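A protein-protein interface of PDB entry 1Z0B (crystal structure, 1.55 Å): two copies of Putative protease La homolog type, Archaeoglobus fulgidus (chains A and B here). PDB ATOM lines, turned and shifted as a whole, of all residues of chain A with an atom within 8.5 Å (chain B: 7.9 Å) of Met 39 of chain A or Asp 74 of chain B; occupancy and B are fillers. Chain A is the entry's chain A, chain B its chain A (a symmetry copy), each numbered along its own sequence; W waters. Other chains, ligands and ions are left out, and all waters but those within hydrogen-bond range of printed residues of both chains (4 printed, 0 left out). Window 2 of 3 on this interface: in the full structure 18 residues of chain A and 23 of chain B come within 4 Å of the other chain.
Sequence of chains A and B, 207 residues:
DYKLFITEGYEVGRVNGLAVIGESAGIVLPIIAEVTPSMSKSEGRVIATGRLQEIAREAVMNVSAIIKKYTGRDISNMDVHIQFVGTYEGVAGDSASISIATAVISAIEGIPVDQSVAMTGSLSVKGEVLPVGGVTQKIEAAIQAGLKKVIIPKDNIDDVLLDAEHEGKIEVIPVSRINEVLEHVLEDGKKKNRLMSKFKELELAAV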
ATOM      1  N   THR A  36     -10.864 -17.467 -17.549  1.00  0.00           N
ATOM      2  CA  THR A  36      -9.991 -18.590 -17.806  1.00  0.00           C
ATOM      3  C   THR A  36     -10.480 -19.318 -19.054  1.00  0.00           C
ATOM      4  O   THR A  36     -11.612 -19.137 -19.480  1.00  0.00           O
ATOM      5  CB  THR A  36     -10.013 -19.607 -16.640  1.00  0.00           C
ATOM      6  OG1 THR A  36     -11.217 -20.384 -16.673  1.00  0.00           O
ATOM      7  CG2 THR A  36      -9.948 -18.915 -15.304  1.00  0.00           C
ATOM      8  N   PRO A  37      -9.650 -20.213 -19.623  1.00  0.00           N
ATOM      9  CA  PRO A  37     -10.187 -21.120 -20.642  1.00  0.00           C
ATOM     10  C   PRO A  37     -11.228 -22.071 -20.057  1.00  0.00           C
ATOM     11  O   PRO A  37     -11.194 -22.367 -18.847  1.00  0.00           O
ATOM     12  CB  PRO A  37      -8.946 -21.907 -21.077  1.00  0.00           C
ATOM     13  CG  PRO A  37      -7.795 -21.004 -20.712  1.00  0.00           C
ATOM     14  CD  PRO A  37      -8.216 -20.452 -19.393  1.00  0.00           C
ATOM     15  N   SER A  38     -12.179 -22.514 -20.880  1.00  0.00           N
ATOM     16  CA  SER A  38     -13.260 -23.364 -20.388  1.00  0.00           C
ATOM     17  C   SER A  38     -12.893 -24.853 -20.256  1.00  0.00           C
ATOM     18  O   SER A  38     -13.687 -25.651 -19.736  1.00  0.00           O
ATOM     19  CB  SER A  38     -14.497 -23.181 -21.254  1.00  0.00           C
ATOM     20  OG  SER A  38     -14.148 -23.394 -22.613  1.00  0.00           O
ATOM     21  N   MET A  39     -11.699 -25.238 -20.704  1.00  0.00           N
ATOM     22  CA  MET A  39     -11.177 -26.622 -20.478  1.00  0.00           C
ATOM     23  C   MET A  39     -12.045 -27.778 -20.986  1.00  0.00           C
ATOM     24  O   MET A  39     -12.831 -27.622 -21.927  1.00  0.00           O
ATOM     25  CB  MET A  39     -10.923 -26.871 -18.987  1.00  0.00           C
ATOM     26  CG  MET A  39     -10.244 -25.731 -18.244  1.00  0.00           C
ATOM     27  SD  MET A  39      -8.523 -25.598 -18.688  1.00  0.00           S
ATOM     28  CE  MET A  39      -7.885 -27.107 -17.961  1.00  0.00           C
ATOM     29  N   GLU A  43     -17.976 -24.795 -23.992  1.00  0.00           N
ATOM     30  CA  GLU A  43     -18.804 -23.649 -23.632  1.00  0.00           C
ATOM     31  C   GLU A  43     -18.427 -23.090 -22.262  1.00  0.00           C
ATOM     32  O   GLU A  43     -18.402 -23.831 -21.285  1.00  0.00           O
ATOM     33  CB  GLU A  43     -20.277 -24.045 -23.605  1.00  0.00           C
ATOM     34  CG  GLU A  43     -21.256 -22.860 -23.536  1.00  0.00           C
ATOM     35  CD  GLU A  43     -21.932 -22.553 -24.872  1.00  0.00           C
ATOM     36  OE1 GLU A  43     -22.493 -23.484 -25.509  1.00  0.00           O
ATOM     37  OE2 GLU A  43     -21.910 -21.363 -25.276  1.00  0.00           O
ATOM     38  N   GLY A  44     -18.169 -21.781 -22.207  1.00  0.00           N
ATOM     39  CA  GLY A  44     -17.817 -21.089 -20.964  1.00  0.00           C
ATOM     40  C   GLY A  44     -18.974 -20.871 -20.001  1.00  0.00           C
ATOM     41  O   GLY A  44     -20.122 -20.729 -20.428  1.00  0.00           O
ATOM     42  N   ARG A  45     -18.666 -20.847 -18.701  1.00  0.00           N
ATOM     43  CA  ARG A  45     -19.655 -20.611 -17.643  1.00  0.00           C
ATOM     44  C   ARG A  45     -19.394 -19.281 -16.942  1.00  0.00           C
ATOM     45  O   ARG A  45     -18.249 -18.877 -16.823  1.00  0.00           O
ATOM     46  CB  ARG A  45     -19.538 -21.685 -16.563  1.00  0.00           C
ATOM     47  CG  ARG A  45     -20.361 -22.936 -16.755  1.00  0.00           C
ATOM     48  CD  ARG A  45     -20.577 -23.606 -15.363  1.00  0.00           C
ATOM     49  NE  ARG A  45     -19.410 -24.379 -14.882  1.00  0.00           N
ATOM     50  CZ  ARG A  45     -19.110 -24.648 -13.595  1.00  0.00           C
ATOM     51  NH1 ARG A  45     -19.859 -24.195 -12.576  1.00  0.00           N
ATOM     52  NH2 ARG A  45     -18.023 -25.374 -13.324  1.00  0.00           N
ATOM     53  N   ASN A  77     -16.043 -18.972 -24.991  1.00  0.00           N
ATOM     54  CA  ASN A  77     -15.205 -20.114 -24.654  1.00  0.00           C
ATOM     55  C   ASN A  77     -14.287 -19.834 -23.479  1.00  0.00           C
ATOM     56  O   ASN A  77     -13.230 -20.459 -23.323  1.00  0.00           O
ATOM     57  CB  ASN A  77     -14.427 -20.600 -25.878  1.00  0.00           C
ATOM     58  CG  ASN A  77     -15.151 -21.720 -26.574  1.00  0.00           C
ATOM     59  OD1 ASN A  77     -15.102 -22.879 -26.124  1.00  0.00           O
ATOM     60  ND2 ASN A  77     -15.882 -21.386 -27.640  1.00  0.00           N
ATOM     61  N   MET A  78     -14.702 -18.879 -22.649  1.00  0.00           N
ATOM     62  CA  MET A  78     -13.998 -18.630 -21.421  1.00  0.00           C
ATOM     63  C   MET A  78     -14.941 -18.833 -20.251  1.00  0.00           C
ATOM     64  O   MET A  78     -16.140 -18.602 -20.363  1.00  0.00           O
ATOM     65  CB  MET A  78     -13.471 -17.209 -21.397  1.00  0.00           C
ATOM     66  CG  MET A  78     -12.515 -16.862 -22.506  1.00  0.00           C
ATOM     67  SD  MET A  78     -12.213 -15.095 -22.454  1.00  0.00           S
ATOM     68  CE  MET A  78     -11.535 -14.799 -24.083  1.00  0.00           C
ATOM     69  N   ASP A  79     -14.386 -19.266 -19.122  1.00  0.00           N
ATOM     70  CA  ASP A  79     -15.111 -19.178 -17.866  1.00  0.00           C
ATOM     71  C   ASP A  79     -14.867 -17.778 -17.284  1.00  0.00           C
ATOM     72  O   ASP A  79     -13.754 -17.240 -17.343  1.00  0.00           O
ATOM     73  CB  ASP A  79     -14.625 -20.237 -16.882  1.00  0.00           C
ATOM     74  CG  ASP A  79     -15.038 -21.635 -17.274  1.00  0.00           C
ATOM     75  OD1 ASP A  79     -15.999 -21.820 -18.057  1.00  0.00           O
ATOM     76  OD2 ASP A  79     -14.392 -22.582 -16.787  1.00  0.00           O
ATOM     77  N   THR B  36     -12.690 -35.826  -6.923  1.00  0.00           N
ATOM     78  CA  THR B  36     -12.972 -37.077  -7.591  1.00  0.00           C
ATOM     79  C   THR B  36     -13.393 -36.783  -9.028  1.00  0.00           C
ATOM     80  O   THR B  36     -13.752 -35.660  -9.357  1.00  0.00           O
ATOM     81  CB  THR B  36     -14.139 -37.835  -6.914  1.00  0.00           C
ATOM     82  OG1 THR B  36     -15.394 -37.234  -7.256  1.00  0.00           O
ATOM     83  CG2 THR B  36     -14.010 -37.816  -5.413  1.00  0.00           C
ATOM     84  N   SER B  38     -16.183 -36.643 -11.966  1.00  0.00           N
ATOM     85  CA  SER B  38     -17.596 -36.293 -11.851  1.00  0.00           C
ATOM     86  C   SER B  38     -18.567 -37.397 -12.308  1.00  0.00           C
ATOM     87  O   SER B  38     -19.788 -37.265 -12.145  1.00  0.00           O
ATOM     88  CB  SER B  38     -17.868 -34.989 -12.585  1.00  0.00           C
ATOM     89  OG  SER B  38     -17.392 -35.097 -13.918  1.00  0.00           O
ATOM     90  N   GLY B  44     -18.551 -31.019 -12.940  1.00  0.00           N
ATOM     91  CA  GLY B  44     -18.232 -31.218 -11.523  1.00  0.00           C
ATOM     92  C   GLY B  44     -19.030 -30.352 -10.559  1.00  0.00           C
ATOM     93  O   GLY B  44     -19.425 -29.237 -10.904  1.00  0.00           O
ATOM     94  N   SER B  64     -10.550 -22.624  -8.233  1.00  0.00           N
ATOM     95  CA  SER B  64     -10.708 -23.247  -9.535  1.00  0.00           C
ATOM     96  C   SER B  64     -10.215 -22.318 -10.621  1.00  0.00           C
ATOM     97  O   SER B  64      -9.594 -22.781 -11.573  1.00  0.00           O
ATOM     98  CB  SER B  64     -12.150 -23.603  -9.781  1.00  0.00           C
ATOM     99  OG  SER B  64     -12.471 -24.724  -8.961  1.00  0.00           O
ATOM    100  N   ILE B  67      -6.461 -22.543 -10.630  1.00  0.00           N
ATOM    101  CA  ILE B  67      -6.043 -23.896 -11.020  1.00  0.00           C
ATOM    102  C   ILE B  67      -6.165 -24.035 -12.525  1.00  0.00           C
ATOM    103  O   ILE B  67      -5.225 -24.509 -13.165  1.00  0.00           O
ATOM    104  CB  ILE B  67      -6.844 -24.987 -10.273  1.00  0.00           C
ATOM    105  CG1 ILE B  67      -6.351 -25.045  -8.837  1.00  0.00           C
ATOM    106  CG2 ILE B  67      -6.720 -26.341 -10.966  1.00  0.00           C
ATOM    107  CD1 ILE B  67      -7.247 -25.855  -7.901  1.00  0.00           C
ATOM    108  N   LYS B  68      -7.304 -23.628 -13.086  1.00  0.00           N
ATOM    109  CA  LYS B  68      -7.493 -23.686 -14.537  1.00  0.00           C
ATOM    110  C   LYS B  68      -6.475 -22.846 -15.264  1.00  0.00           C
ATOM    111  O   LYS B  68      -5.810 -23.323 -16.194  1.00  0.00           O
ATOM    112  CB  LYS B  68      -8.917 -23.299 -14.929  1.00  0.00           C
ATOM    113  CG  LYS B  68      -9.959 -24.316 -14.459  1.00  0.00           C
ATOM    114  CD  LYS B  68     -11.358 -23.926 -14.893  1.00  0.00           C
ATOM    115  CE  LYS B  68     -11.820 -22.667 -14.153  1.00  0.00           C
ATOM    116  NZ  LYS B  68     -13.255 -22.387 -14.420  1.00  0.00           N
ATOM    117  N   LYS B  69      -6.305 -21.608 -14.832  1.00  0.00           N
ATOM    118  CA  LYS B  69      -5.463 -20.673 -15.554  1.00  0.00           C
ATOM    119  C   LYS B  69      -4.006 -21.083 -15.511  1.00  0.00           C
ATOM    120  O   LYS B  69      -3.333 -21.071 -16.541  1.00  0.00           O
ATOM    121  CB  LYS B  69      -5.647 -19.272 -14.971  1.00  0.00           C
ATOM    122  CG  LYS B  69      -5.037 -18.196 -15.790  1.00  0.00           C
ATOM    123  CD  LYS B  69      -5.480 -16.839 -15.316  1.00  0.00           C
ATOM    124  CE  LYS B  69      -4.640 -15.758 -16.005  1.00  0.00           C
ATOM    125  NZ  LYS B  69      -5.227 -14.404 -15.861  1.00  0.00           N
ATOM    126  N   TYR B  70      -3.510 -21.456 -14.345  1.00  0.00           N
ATOM    127  CA  TYR B  70      -2.061 -21.596 -14.156  1.00  0.00           C
ATOM    128  C   TYR B  70      -1.534 -23.014 -14.107  1.00  0.00           C
ATOM    129  O   TYR B  70      -0.339 -23.222 -14.323  1.00  0.00           O
ATOM    130  CB  TYR B  70      -1.637 -20.858 -12.892  1.00  0.00           C
ATOM    131  CG  TYR B  70      -1.810 -19.383 -13.026  1.00  0.00           C
ATOM    132  CD1 TYR B  70      -0.958 -18.640 -13.835  1.00  0.00           C
ATOM    133  CD2 TYR B  70      -2.827 -18.726 -12.366  1.00  0.00           C
ATOM    134  CE1 TYR B  70      -1.111 -17.266 -13.981  1.00  0.00           C
ATOM    135  CE2 TYR B  70      -2.998 -17.355 -12.494  1.00  0.00           C
ATOM    136  CZ  TYR B  70      -2.134 -16.617 -13.294  1.00  0.00           C
ATOM    137  OH  TYR B  70      -2.306 -15.246 -13.385  1.00  0.00           O
ATOM    138  N   THR B  71      -2.401 -23.981 -13.786  1.00  0.00           N
ATOM    139  CA  THR B  71      -1.942 -25.366 -13.659  1.00  0.00           C
ATOM    140  C   THR B  71      -2.561 -26.278 -14.718  1.00  0.00           C
ATOM    141  O   THR B  71      -2.051 -27.365 -14.972  1.00  0.00           O
ATOM    142  CB  THR B  71      -2.142 -25.951 -12.223  1.00  0.00           C
ATOM    143  OG1 THR B  71      -3.517 -26.299 -12.023  1.00  0.00           O
ATOM    144  CG2 THR B  71      -1.674 -24.990 -11.138  1.00  0.00           C
ATOM    145  N   GLY B  72      -3.661 -25.832 -15.317  1.00  0.00           N
ATOM    146  CA  GLY B  72      -4.320 -26.583 -16.363  1.00  0.00           C
ATOM    147  C   GLY B  72      -5.023 -27.855 -15.923  1.00  0.00           C
ATOM    148  O   GLY B  72      -5.397 -28.674 -16.775  1.00  0.00           O
ATOM    149  N   ARG B  73      -5.230 -28.055 -14.618  1.00  0.00           N
ATOM    150  CA  ARG B  73      -6.055 -29.215 -14.187  1.00  0.00           C
ATOM    151  C   ARG B  73      -7.496 -28.951 -14.557  1.00  0.00           C
ATOM    152  O   ARG B  73      -8.001 -27.850 -14.335  1.00  0.00           O
ATOM    153  CB  ARG B  73      -5.959 -29.451 -12.690  1.00  0.00           C
ATOM    154  CG  ARG B  73      -4.539 -29.666 -12.166  1.00  0.00           C
ATOM    155  CD  ARG B  73      -3.894 -30.927 -12.731  1.00  0.00           C
ATOM    156  NE  ARG B  73      -2.698 -31.297 -11.974  1.00  0.00           N
ATOM    157  CZ  ARG B  73      -1.603 -31.865 -12.494  1.00  0.00           C
ATOM    158  NH1 ARG B  73      -1.523 -32.131 -13.802  1.00  0.00           N
ATOM    159  NH2 ARG B  73      -0.565 -32.153 -11.708  1.00  0.00           N
ATOM    160  N   ASP B  74      -8.163 -29.956 -15.116  1.00  0.00           N
ATOM    161  CA  ASP B  74      -9.546 -29.806 -15.553  1.00  0.00           C
ATOM    162  C   ASP B  74     -10.464 -29.933 -14.330  1.00  0.00           C
ATOM    163  O   ASP B  74     -11.276 -30.856 -14.244  1.00  0.00           O
ATOM    164  CB  ASP B  74      -9.870 -30.897 -16.583  1.00  0.00           C
ATOM    165  CG  ASP B  74     -11.222 -30.704 -17.251  1.00  0.00           C
ATOM    166  OD1 ASP B  74     -11.769 -29.587 -17.211  1.00  0.00           O
ATOM    167  OD2 ASP B  74     -11.752 -31.687 -17.820  1.00  0.00           O
ATOM    168  N   ILE B  75     -10.339 -29.016 -13.386  1.00  0.00           N
ATOM    169  CA  ILE B  75     -11.121 -29.082 -12.150  1.00  0.00           C
ATOM    170  C   ILE B  75     -12.635 -28.972 -12.414  1.00  0.00           C
ATOM    171  O   ILE B  75     -13.448 -29.420 -11.596  1.00  0.00           O
ATOM    172  CB  ILE B  75     -10.591 -28.054 -11.123  1.00  0.00           C
ATOM    173  CG1 ILE B  75     -11.183 -28.294  -9.709  1.00  0.00           C
ATOM    174  CG2 ILE B  75     -10.790 -26.615 -11.641  1.00  0.00           C
ATOM    175  CD1 ILE B  75     -10.541 -27.452  -8.632  1.00  0.00           C
ATOM    176  N   SER B  76     -13.018 -28.417 -13.570  1.00  0.00           N
ATOM    177  CA  SER B  76     -14.431 -28.336 -13.978  1.00  0.00           C
ATOM    178  C   SER B  76     -15.112 -29.696 -14.156  1.00  0.00           C
ATOM    179  O   SER B  76     -16.348 -29.795 -14.124  1.00  0.00           O
ATOM    180  CB  SER B  76     -14.549 -27.584 -15.303  1.00  0.00           C
ATOM    181  OG  SER B  76     -13.853 -26.357 -15.233  1.00  0.00           O
ATOM    182  N   ASN B  77     -14.313 -30.728 -14.396  1.00  0.00           N
ATOM    183  CA  ASN B  77     -14.823 -32.086 -14.525  1.00  0.00           C
ATOM    184  C   ASN B  77     -14.477 -32.952 -13.328  1.00  0.00           C
ATOM    185  O   ASN B  77     -14.411 -34.184 -13.421  1.00  0.00           O
ATOM    186  CB  ASN B  77     -14.357 -32.721 -15.837  1.00  0.00           C
ATOM    187  CG  ASN B  77     -15.388 -32.552 -16.919  1.00  0.00           C
ATOM    188  OD1 ASN B  77     -16.390 -33.290 -16.956  1.00  0.00           O
ATOM    189  ND2 ASN B  77     -15.197 -31.546 -17.775  1.00  0.00           N
ATOM    190  N   MET B  78     -14.253 -32.291 -12.193  1.00  0.00           N
ATOM    191  CA  MET B  78     -14.070 -33.007 -10.961  1.00  0.00           C
ATOM    192  C   MET B  78     -15.136 -32.581  -9.969  1.00  0.00           C
ATOM    193  O   MET B  78     -15.595 -31.445  -9.990  1.00  0.00           O
ATOM    194  CB  MET B  78     -12.701 -32.712 -10.382  1.00  0.00           C
ATOM    195  CG  MET B  78     -11.540 -33.086 -11.262  1.00  0.00           C
ATOM    196  SD  MET B  78     -10.042 -32.431 -10.523  1.00  0.00           S
ATOM    197  CE  MET B  78      -8.905 -32.491 -11.904  1.00  0.00           C
ATOM    198  N   ASP B  79     -15.521 -33.507  -9.095  1.00  0.00           N
ATOM    199  CA  ASP B  79     -16.270 -33.129  -7.908  1.00  0.00           C
ATOM    200  C   ASP B  79     -15.259 -32.730  -6.825  1.00  0.00           C
ATOM    201  O   ASP B  79     -14.205 -33.360  -6.662  1.00  0.00           O
ATOM    202  CB  ASP B  79     -17.125 -34.291  -7.413  1.00  0.00           C
ATOM    203  CG  ASP B  79     -18.293 -34.590  -8.321  1.00  0.00           C
ATOM    204  OD1 ASP B  79     -18.717 -33.723  -9.120  1.00  0.00           O
ATOM    205  OD2 ASP B  79     -18.810 -35.721  -8.238  1.00  0.00           O
ATOM    206  N   ILE B 108      -5.669 -32.124  -5.162  1.00  0.00           N
ATOM    207  CA  ILE B 108      -5.581 -32.355  -6.610  1.00  0.00           C
ATOM    208  C   ILE B 108      -4.165 -32.738  -6.985  1.00  0.00           C
ATOM    209  O   ILE B 108      -3.995 -33.559  -7.876  1.00  0.00           O
ATOM    210  CB  ILE B 108      -6.042 -31.149  -7.474  1.00  0.00           C
ATOM    211  CG1 ILE B 108      -7.456 -30.753  -7.168  1.00  0.00           C
ATOM    212  CG2 ILE B 108      -6.006 -31.510  -8.957  1.00  0.00           C
ATOM    213  CD1 ILE B 108      -7.804 -29.449  -7.797  1.00  0.00           C
HETATM  214  O   HOH W   1     -16.722 -24.679 -16.202  1.00  0.00           O
HETATM  215  O   HOH W   2     -17.664 -27.210 -11.392  1.00  0.00           O
HETATM  216  O   HOH W   3     -14.744 -24.524 -12.891  1.00  0.00           O
HETATM  217  O   HOH W   4     -14.074 -25.206 -17.382  1.00  0.00           O
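The side-chain amino group (NZ) of Lys 68 of chain B lies within salt-bridge range of the side-chain carboxylate (OD2) of Asp 79 of chain A (2.6 Å).
The backbone carbonyl oxygen (O) of Thr 36 of chain A sits at hydrogen-bond distance from the backbone NH (N) of Asp 79 of chain A (2.8 Å).
OD1 of Asp 79 of chain A lies within hydrogen-bond range of N of Arg 45 of chain A, at 2.9 Å.
The backbone carbonyl oxygen of Ile 67 of chain B sits at hydrogen-bond distance from the backbone NH of Gly 72 of chain B (3.0 Å).
ND2 of Asn 77 of chain B sits close to OD2 of Asp 74 of chain B (3.4 Å).
Thr 36 of chain A touches Lys 68 of chain B (OG1 to CE, 3.5 Å).
Met 39 of chain A touches Lys 68 of chain B.
Gly 72 of chain B touches Met 39 of chain A (O to CE, 3.2 Å).
Met 39 of chain A touches Arg 73 of chain B (CE to O, 3.7 Å).
Asp 74 of chain B touches Met 39 of chain A.
Printed residues of chain B within 4 Å of Thr 36 of chain A: Lys 68 (3.5 Å).
Met 78 of chain A touches none of the printed residues of chain B.
Of the printed residues of chain B, Asp 79 of chain A touches Lys 68.
Printed residues of chain A within 4 Å of Lys 68 of chain B: Thr 36 (3.5 Å), Met 39 (3.97 Å) and Asp 79 (2.6 Å).
Of the printed residues of chain A, Gly 72 of chain B touches Met 39 (3.2 Å).
Asp 74 of chain B touches just one residue of chain A: Met 39.
The nearest residue of chain B that does not touch Met 39 of chain A is Ser 76 of chain B (4.7 Å).
The nearest residue of chain A that does not touch Asp 74 of chain B is Ser 38 of chain A (5.1 Å).
Of the 18 printed residues of chain B, 4 touch a printed residue of chain A.
Printed residues of chain B that touch a printed residue of chain A: Lys 68, Gly 72, Arg 73 and Asp 74.
Hydrophobic or aromatic side chains of chain A that line the printed part of chain B: Met 39.
Among the printed residues, Asp or Glu carboxylates within 4 Å of a Lys or Arg side-chain nitrogen of the other chain: Asp 79 of chain A with Lys 68 of chain B (2.6 Å).
6 positions are printed for both chains.
Water W4 lies within hydrogen-bond range of the backbone carbonyl oxygen (O) of Ser 38 of chain A (2.4 Å), the side-chain hydroxyl (OG) of Ser 76 of chain B (2.4 Å) and the side-chain carboxylate (OD2) of Asp 79 of chain A (2.7 Å).
Water W2 bridges the guanidinium group (NH2) of Arg 45 of chain A and the backbone carbonyl oxygen (O) of Gly 44 of chain B.
Water W1 lies within hydrogen-bond range of NE of Arg 45 of chain A, OD2 of Asp 79 of chain A and OG of Ser 76 of chain B.
Water W3 lies within hydrogen-bond range of the side-chain amino group (NZ) of Lys 68 of chain B (3.0 Å), the side-chain hydroxyl (OG) of Ser 76 of chain B (3.1 Å) and the guanidinium group (NH2) of Arg 45 of chain A (3.4 Å).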
